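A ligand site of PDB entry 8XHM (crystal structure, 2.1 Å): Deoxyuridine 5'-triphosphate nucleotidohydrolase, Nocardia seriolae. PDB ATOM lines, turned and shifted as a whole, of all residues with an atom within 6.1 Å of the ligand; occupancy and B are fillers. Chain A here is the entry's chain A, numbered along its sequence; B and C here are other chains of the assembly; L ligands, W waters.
An oxygen (O2) of the ligand lies close to the backbone carbonyl oxygen (O) of Gly 143 of chain B (3.4 Å).
Merely in contact with the ligand: Gly 141 of chain B, Thr 83, Tyr 88, Gly 82, Ile 63, Tyr 142 of chain B, Ile 92, Ser 67 of chain C, Gly 140 of chain B and Val 84.
Along chain A the residues within 4 Å of the ligand span positions 63 to 93.
The side-chain hydroxyl of Tyr 88 is in hydrogen-bond range of the backbone carbonyl oxygen of Glu 91 (2.6 Å).
OG1 of Thr 83 sits at hydrogen-bond distance from O of Pro 81 (3.2 Å).
The guanidinium group (NH1) of Arg 137 of chain B sits at hydrogen-bond distance from the backbone carbonyl oxygen (O) of Gly 140 of chain B (2.8 Å).
O of Gly 82 sits at hydrogen-bond distance from N of Ile 63 (2.8 Å).
The guanidinium group (NE) of Arg 137 of chain B is in salt-bridge range of the side-chain carboxylate (OD1) of Asp 26 of chain C (3.0 Å).
OD2 of Asp 85 is in salt-bridge range of NH2 of Arg 137 of chain B, at 3.4 Å.
The backbone carbonyl oxygen of Lys 93 sits at hydrogen-bond distance from a nitrogen (N2) of the ligand (2.6 Å).
O3 of the ligand is in hydrogen-bond range of OD2 of Asp 85 (2.6 Å).
An oxygen (O3) of the ligand is in hydrogen-bond range of the backbone NH (N) of Asp 85, 3.0 Å away.
The side-chain amide nitrogen of Asn 79 lies within hydrogen-bond range of an oxygen (O2) of the ligand, at 3.1 Å.
O1 of the ligand sits at hydrogen-bond distance from N of Lys 93, 3.0 Å away.
O7 of the ligand lies within salt-bridge range of NH1 of Arg 137 of chain B (2.9 Å).
Water W3 lies within hydrogen-bond range of the backbone NH of Gly 68 of chain C, an oxygen (O8) of the ligand and the backbone NH of Ser 67 of chain C.
Water W1 lies within hydrogen-bond range of OG of Ser 67 of chain C, N of Thr 83 and ND2 of Asn 79.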
ATOM      1  N   ILE A  63      20.367 -33.258   4.004  1.00  0.00           N
ATOM      2  CA  ILE A  63      21.800 -33.031   4.200  1.00  0.00           C
ATOM      3  C   ILE A  63      22.433 -34.365   4.580  1.00  0.00           C
ATOM      4  O   ILE A  63      22.152 -34.925   5.640  1.00  0.00           O
ATOM      5  CB  ILE A  63      22.045 -31.957   5.265  1.00  0.00           C
ATOM      6  CG1 ILE A  63      21.437 -30.622   4.811  1.00  0.00           C
ATOM      7  CG2 ILE A  63      23.523 -31.795   5.583  1.00  0.00           C
ATOM      8  CD1 ILE A  63      21.371 -29.588   5.906  1.00  0.00           C
ATOM      9  N   VAL A  77      27.428 -36.350  10.357  1.00  0.00           N
ATOM     10  CA  VAL A  77      26.398 -35.355  10.683  1.00  0.00           C
ATOM     11  C   VAL A  77      25.506 -35.949  11.763  1.00  0.00           C
ATOM     12  O   VAL A  77      24.985 -37.064  11.595  1.00  0.00           O
ATOM     13  CB  VAL A  77      25.589 -34.983   9.415  1.00  0.00           C
ATOM     14  CG1 VAL A  77      24.359 -34.111   9.743  1.00  0.00           C
ATOM     15  CG2 VAL A  77      26.486 -34.307   8.364  1.00  0.00           C
ATOM     16  N   ASN A  79      22.484 -35.237  13.178  1.00  0.00           N
ATOM     17  CA  ASN A  79      21.078 -35.430  12.833  1.00  0.00           C
ATOM     18  C   ASN A  79      20.899 -35.970  11.419  1.00  0.00           C
ATOM     19  O   ASN A  79      19.873 -35.677  10.780  1.00  0.00           O
ATOM     20  CB  ASN A  79      20.311 -34.111  12.990  1.00  0.00           C
ATOM     21  CG  ASN A  79      20.816 -33.040  12.036  1.00  0.00           C
ATOM     22  OD1 ASN A  79      22.016 -32.890  11.829  1.00  0.00           O
ATOM     23  ND2 ASN A  79      19.894 -32.281  11.477  1.00  0.00           N
ATOM     24  N   PRO A  81      19.820 -38.032   8.219  1.00  0.00           N
ATOM     25  CA  PRO A  81      19.932 -37.030   7.157  1.00  0.00           C
ATOM     26  C   PRO A  81      19.351 -35.710   7.650  1.00  0.00           C
ATOM     27  O   PRO A  81      18.221 -35.699   8.151  1.00  0.00           O
ATOM     28  CB  PRO A  81      19.154 -37.670   5.994  1.00  0.00           C
ATOM     29  CG  PRO A  81      18.111 -38.489   6.666  1.00  0.00           C
ATOM     30  CD  PRO A  81      18.753 -39.015   7.929  1.00  0.00           C
ATOM     31  N   GLY A  82      20.091 -34.597   7.587  1.00  0.00           N
ATOM     32  CA  GLY A  82      19.545 -33.327   8.045  1.00  0.00           C
ATOM     33  C   GLY A  82      18.351 -32.931   7.195  1.00  0.00           C
ATOM     34  O   GLY A  82      18.430 -32.975   5.970  1.00  0.00           O
ATOM     35  N   THR A  83      17.234 -32.536   7.814  1.00  0.00           N
ATOM     36  CA  THR A  83      15.969 -32.334   7.108  1.00  0.00           C
ATOM     37  C   THR A  83      15.672 -30.841   6.979  1.00  0.00           C
ATOM     38  O   THR A  83      15.417 -30.157   7.972  1.00  0.00           O
ATOM     39  CB  THR A  83      14.862 -33.069   7.852  1.00  0.00           C
ATOM     40  OG1 THR A  83      15.243 -34.444   7.984  1.00  0.00           O
ATOM     41  CG2 THR A  83      13.540 -32.975   7.090  1.00  0.00           C
ATOM     42  N   VAL A  84      15.718 -30.325   5.748  1.00  0.00           N
ATOM     43  CA  VAL A  84      15.468 -28.920   5.464  1.00  0.00           C
ATOM     44  C   VAL A  84      14.058 -28.796   4.909  1.00  0.00           C
ATOM     45  O   VAL A  84      13.775 -29.288   3.816  1.00  0.00           O
ATOM     46  CB  VAL A  84      16.487 -28.345   4.464  1.00  0.00           C
ATOM     47  CG1 VAL A  84      16.152 -26.899   4.150  1.00  0.00           C
ATOM     48  CG2 VAL A  84      17.917 -28.499   4.998  1.00  0.00           C
ATOM     49  N   ASP A  85      13.162 -28.124   5.638  1.00  0.00           N
ATOM     50  CA  ASP A  85      11.766 -28.080   5.252  1.00  0.00           C
ATOM     51  C   ASP A  85      11.527 -27.055   4.147  1.00  0.00           C
ATOM     52  O   ASP A  85      12.274 -26.078   4.002  1.00  0.00           O
ATOM     53  CB  ASP A  85      10.888 -27.764   6.472  1.00  0.00           C
ATOM     54  CG  ASP A  85      10.987 -28.837   7.545  1.00  0.00           C
ATOM     55  OD1 ASP A  85      10.461 -29.955   7.335  1.00  0.00           O
ATOM     56  OD2 ASP A  85      11.599 -28.576   8.599  1.00  0.00           O
ATOM     57  N   ALA A  86      10.474 -27.295   3.347  1.00  0.00           N
ATOM     58  CA  ALA A  86      10.161 -26.415   2.219  1.00  0.00           C
ATOM     59  C   ALA A  86       9.953 -24.972   2.655  1.00  0.00           C
ATOM     60  O   ALA A  86      10.345 -24.043   1.945  1.00  0.00           O
ATOM     61  CB  ALA A  86       8.925 -26.923   1.474  1.00  0.00           C
ATOM     62  N   TYR A  88      11.385 -23.383   5.083  1.00  0.00           N
ATOM     63  CA  TYR A  88      12.513 -22.804   5.791  1.00  0.00           C
ATOM     64  C   TYR A  88      13.175 -21.726   4.955  1.00  0.00           C
ATOM     65  O   TYR A  88      13.483 -21.936   3.782  1.00  0.00           O
ATOM     66  CB  TYR A  88      13.545 -23.883   6.121  1.00  0.00           C
ATOM     67  CG  TYR A  88      14.712 -23.384   6.939  1.00  0.00           C
ATOM     68  CD1 TYR A  88      14.547 -22.962   8.250  1.00  0.00           C
ATOM     69  CD2 TYR A  88      15.998 -23.339   6.388  1.00  0.00           C
ATOM     70  CE1 TYR A  88      15.631 -22.521   9.010  1.00  0.00           C
ATOM     71  CE2 TYR A  88      17.087 -22.915   7.134  1.00  0.00           C
ATOM     72  CZ  TYR A  88      16.890 -22.499   8.449  1.00  0.00           C
ATOM     73  OH  TYR A  88      17.973 -22.053   9.187  1.00  0.00           O
ATOM     74  N   GLU A  91      19.420 -19.510   7.092  1.00  0.00           N
ATOM     75  CA  GLU A  91      20.677 -20.088   6.630  1.00  0.00           C
ATOM     76  C   GLU A  91      20.694 -21.585   6.912  1.00  0.00           C
ATOM     77  O   GLU A  91      20.350 -22.013   8.018  1.00  0.00           O
ATOM     78  CB  GLU A  91      21.861 -19.421   7.339  1.00  0.00           C
ATOM     79  CG  GLU A  91      23.216 -19.886   6.800  1.00  0.00           C
ATOM     80  CD  GLU A  91      24.396 -19.334   7.597  1.00  0.00           C
ATOM     81  OE1 GLU A  91      24.169 -18.627   8.601  1.00  0.00           O
ATOM     82  OE2 GLU A  91      25.564 -19.621   7.214  1.00  0.00           O
ATOM     83  N   ILE A  92      21.117 -22.385   5.937  1.00  0.00           N
ATOM     84  CA  ILE A  92      21.252 -23.816   6.172  1.00  0.00           C
ATOM     85  C   ILE A  92      22.460 -24.057   7.058  1.00  0.00           C
ATOM     86  O   ILE A  92      23.550 -23.531   6.790  1.00  0.00           O
ATOM     87  CB  ILE A  92      21.384 -24.571   4.834  1.00  0.00           C
ATOM     88  CG1 ILE A  92      20.068 -24.489   4.051  1.00  0.00           C
ATOM     89  CG2 ILE A  92      21.796 -26.022   5.090  1.00  0.00           C
ATOM     90  CD1 ILE A  92      20.154 -25.092   2.648  1.00  0.00           C
ATOM     91  N   LYS A  93      22.295 -24.864   8.090  1.00  0.00           N
ATOM     92  CA  LYS A  93      23.389 -25.184   8.988  1.00  0.00           C
ATOM     93  C   LYS A  93      23.601 -26.692   9.042  1.00  0.00           C
ATOM     94  O   LYS A  93      22.684 -27.472   8.755  1.00  0.00           O
ATOM     95  CB  LYS A  93      23.111 -24.596  10.391  1.00  0.00           C
ATOM     96  CG  LYS A  93      22.845 -23.079  10.285  1.00  0.00           C
ATOM     97  CD  LYS A  93      22.687 -22.377  11.616  1.00  0.00           C
ATOM     98  CE  LYS A  93      23.030 -20.891  11.439  1.00  0.00           C
ATOM     99  NZ  LYS A  93      22.538 -20.055  12.575  1.00  0.00           N
ATOM    100  N   VAL A  94      24.821 -27.092   9.376  1.00  0.00           N
ATOM    101  CA  VAL A  94      25.197 -28.502   9.440  1.00  0.00           C
ATOM    102  C   VAL A  94      25.759 -28.789  10.821  1.00  0.00           C
ATOM    103  O   VAL A  94      26.687 -28.097  11.271  1.00  0.00           O
ATOM    104  CB  VAL A  94      26.222 -28.858   8.350  1.00  0.00           C
ATOM    105  CG1 VAL A  94      26.603 -30.327   8.433  1.00  0.00           C
ATOM    106  CG2 VAL A  94      25.670 -28.537   6.972  1.00  0.00           C
ATOM    107  N   CYS A  95      25.241 -29.821  11.496  1.00  0.00           N
ATOM    108  CA  CYS A  95      25.746 -30.248  12.794  1.00  0.00           C
ATOM    109  C   CYS A  95      26.730 -31.414  12.609  1.00  0.00           C
ATOM    110  O   CYS A  95      26.317 -32.568  12.489  1.00  0.00           O
ATOM    111  CB  CYS A  95      24.601 -30.651  13.722  1.00  0.00           C
ATOM    112  SG  CYS A  95      25.199 -30.980  15.410  1.00  0.00           S
ATOM    113  N   ARG B 137       6.940 -20.577   8.727  1.00  0.00           N
ATOM    114  CA  ARG B 137       8.033 -21.192   9.477  1.00  0.00           C
ATOM    115  C   ARG B 137       9.185 -20.212   9.673  1.00  0.00           C
ATOM    116  O   ARG B 137       9.733 -20.083  10.780  1.00  0.00           O
ATOM    117  CB  ARG B 137       8.483 -22.458   8.751  1.00  0.00           C
ATOM    118  CG  ARG B 137       9.783 -23.027   9.218  1.00  0.00           C
ATOM    119  CD  ARG B 137      10.023 -24.350   8.534  1.00  0.00           C
ATOM    120  NE  ARG B 137       9.710 -25.490   9.394  1.00  0.00           N
ATOM    121  CZ  ARG B 137      10.395 -25.804  10.486  1.00  0.00           C
ATOM    122  NH1 ARG B 137      11.401 -25.048  10.908  1.00  0.00           N
ATOM    123  NH2 ARG B 137      10.077 -26.905  11.158  1.00  0.00           N
ATOM    124  N   GLY B 140      13.155 -20.145  11.645  1.00  0.00           N
ATOM    125  CA  GLY B 140      13.178 -21.026  12.798  1.00  0.00           C
ATOM    126  C   GLY B 140      13.788 -22.378  12.489  1.00  0.00           C
ATOM    127  O   GLY B 140      13.247 -23.138  11.689  1.00  0.00           O
ATOM    128  N   GLY B 141      14.928 -22.667  13.108  1.00  0.00           N
ATOM    129  CA  GLY B 141      15.588 -23.946  12.917  1.00  0.00           C
ATOM    130  C   GLY B 141      16.742 -24.105  13.874  1.00  0.00           C
ATOM    131  O   GLY B 141      17.278 -23.124  14.401  1.00  0.00           O
ATOM    132  N   TYR B 142      17.123 -25.360  14.104  1.00  0.00           N
ATOM    133  CA  TYR B 142      18.218 -25.715  15.011  1.00  0.00           C
ATOM    134  C   TYR B 142      19.230 -26.614  14.309  1.00  0.00           C
ATOM    135  O   TYR B 142      19.642 -27.661  14.825  1.00  0.00           O
ATOM    136  CB  TYR B 142      17.677 -26.381  16.287  1.00  0.00           C
ATOM    137  CG  TYR B 142      16.876 -25.452  17.171  1.00  0.00           C
ATOM    138  CD1 TYR B 142      17.184 -24.093  17.235  1.00  0.00           C
ATOM    139  CD2 TYR B 142      15.813 -25.924  17.938  1.00  0.00           C
ATOM    140  CE1 TYR B 142      16.452 -23.228  18.038  1.00  0.00           C
ATOM    141  CE2 TYR B 142      15.077 -25.073  18.743  1.00  0.00           C
ATOM    142  CZ  TYR B 142      15.401 -23.727  18.785  1.00  0.00           C
ATOM    143  OH  TYR B 142      14.688 -22.868  19.587  1.00  0.00           O
ATOM    144  N   GLY B 143      19.642 -26.214  13.111  1.00  0.00           N
ATOM    145  CA  GLY B 143      20.613 -26.924  12.284  1.00  0.00           C
ATOM    146  C   GLY B 143      20.878 -28.391  12.572  1.00  0.00           C
ATOM    147  O   GLY B 143      21.929 -28.912  12.192  1.00  0.00           O
ATOM    148  N   ASP C  26       6.053 -28.949   5.767  1.00  0.00           N
ATOM    149  CA  ASP C  26       7.048 -29.634   6.577  1.00  0.00           C
ATOM    150  C   ASP C  26       7.149 -31.097   6.161  1.00  0.00           C
ATOM    151  O   ASP C  26       6.141 -31.761   5.904  1.00  0.00           O
ATOM    152  CB  ASP C  26       6.678 -29.558   8.060  1.00  0.00           C
ATOM    153  CG  ASP C  26       7.254 -28.334   8.748  1.00  0.00           C
ATOM    154  OD1 ASP C  26       7.810 -27.429   8.080  1.00  0.00           O
ATOM    155  OD2 ASP C  26       7.119 -28.273   9.992  1.00  0.00           O
ATOM    156  N   ARG C  66      15.637 -35.630  15.421  1.00  0.00           N
ATOM    157  CA  ARG C  66      15.212 -34.246  15.599  1.00  0.00           C
ATOM    158  C   ARG C  66      16.425 -33.315  15.571  1.00  0.00           C
ATOM    159  O   ARG C  66      17.459 -33.606  16.173  1.00  0.00           O
ATOM    160  CB  ARG C  66      14.458 -34.077  16.924  1.00  0.00           C
ATOM    161  CG  ARG C  66      13.132 -34.833  17.001  1.00  0.00           C
ATOM    162  CD  ARG C  66      11.951 -33.904  17.227  1.00  0.00           C
ATOM    163  NE  ARG C  66      12.154 -33.045  18.385  1.00  0.00           N
ATOM    164  CZ  ARG C  66      11.506 -31.909  18.579  1.00  0.00           C
ATOM    165  NH1 ARG C  66      10.628 -31.455  17.690  1.00  0.00           N
ATOM    166  NH2 ARG C  66      11.733 -31.210  19.676  1.00  0.00           N
ATOM    167  N   SER C  67      16.282 -32.182  14.875  1.00  0.00           N
ATOM    168  CA  SER C  67      17.446 -31.306  14.692  1.00  0.00           C
ATOM    169  C   SER C  67      17.881 -30.675  16.007  1.00  0.00           C
ATOM    170  O   SER C  67      19.075 -30.673  16.326  1.00  0.00           O
ATOM    171  CB  SER C  67      17.128 -30.207  13.662  1.00  0.00           C
ATOM    172  OG  SER C  67      16.305 -30.706  12.607  1.00  0.00           O
ATOM    173  N   GLY C  68      16.937 -30.154  16.790  1.00  0.00           N
ATOM    174  CA  GLY C  68      17.298 -29.420  17.998  1.00  0.00           C
ATOM    175  C   GLY C  68      18.023 -30.282  19.015  1.00  0.00           C
ATOM    176  O   GLY C  68      19.100 -29.929  19.497  1.00  0.00           O
ATOM    177  N   GLN C 115      11.415 -37.640  13.980  1.00  0.00           N
ATOM    178  CA  GLN C 115      10.369 -37.249  13.043  1.00  0.00           C
ATOM    179  C   GLN C 115      10.218 -38.320  11.968  1.00  0.00           C
ATOM    180  O   GLN C 115      11.185 -39.001  11.602  1.00  0.00           O
ATOM    181  CB  GLN C 115      10.658 -35.856  12.422  1.00  0.00           C
ATOM    182  CG  GLN C 115      11.888 -35.802  11.549  1.00  0.00           C
ATOM    183  CD  GLN C 115      12.160 -34.393  11.028  1.00  0.00           C
ATOM    184  OE1 GLN C 115      11.339 -33.829  10.338  1.00  0.00           O
ATOM    185  NE2 GLN C 115      13.319 -33.842  11.357  1.00  0.00           N
HETATM  186  N1  LIG L   1      17.931 -27.276   9.509  1.00  0.00           N
HETATM  187  C1  LIG L   1      19.227 -27.044   9.070  1.00  0.00           C
HETATM  188  N2  LIG L   1      20.141 -28.052   9.015  1.00  0.00           N
HETATM  189  C2  LIG L   1      19.827 -29.309   9.406  1.00  0.00           C
HETATM  190  C3  LIG L   1      18.510 -29.548   9.862  1.00  0.00           C
HETATM  191  C4  LIG L   1      17.579 -28.522   9.903  1.00  0.00           C
HETATM  192  O1  LIG L   1      19.585 -25.935   8.707  1.00  0.00           O
HETATM  193  O2  LIG L   1      20.679 -30.204   9.356  1.00  0.00           O
HETATM  194  C5  LIG L   1      16.989 -26.169   9.523  1.00  0.00           C
HETATM  195  C6  LIG L   1      16.023 -26.270   8.317  1.00  0.00           C
HETATM  196  C7  LIG L   1      14.797 -26.954   8.969  1.00  0.00           C
HETATM  197  C8  LIG L   1      14.807 -26.373  10.342  1.00  0.00           C
HETATM  198  O3  LIG L   1      13.477 -26.829   8.362  1.00  0.00           O
HETATM  199  O4  LIG L   1      16.197 -26.230  10.671  1.00  0.00           O
HETATM  200  C9  LIG L   1      14.106 -27.441  11.182  1.00  0.00           C
HETATM  201  O5  LIG L   1      14.458 -27.228  12.510  1.00  0.00           O
HETATM  202  P1  LIG L   1      13.296 -27.445  13.611  1.00  0.00           P
HETATM  203  O6  LIG L   1      13.870 -26.991  14.932  1.00  0.00           O
HETATM  204  O7  LIG L   1      12.164 -26.566  13.236  1.00  0.00           O
HETATM  205  O8  LIG L   1      12.919 -28.914  13.462  1.00  0.00           O
HETATM  206  O   HOH W   1      17.067 -32.566  10.646  1.00  0.00           O
HETATM  207  O   HOH W   2      23.098 -31.133  10.072  1.00  0.00           O
HETATM  208  O   HOH W   3      13.921 -30.016  16.274  1.00  0.00           O
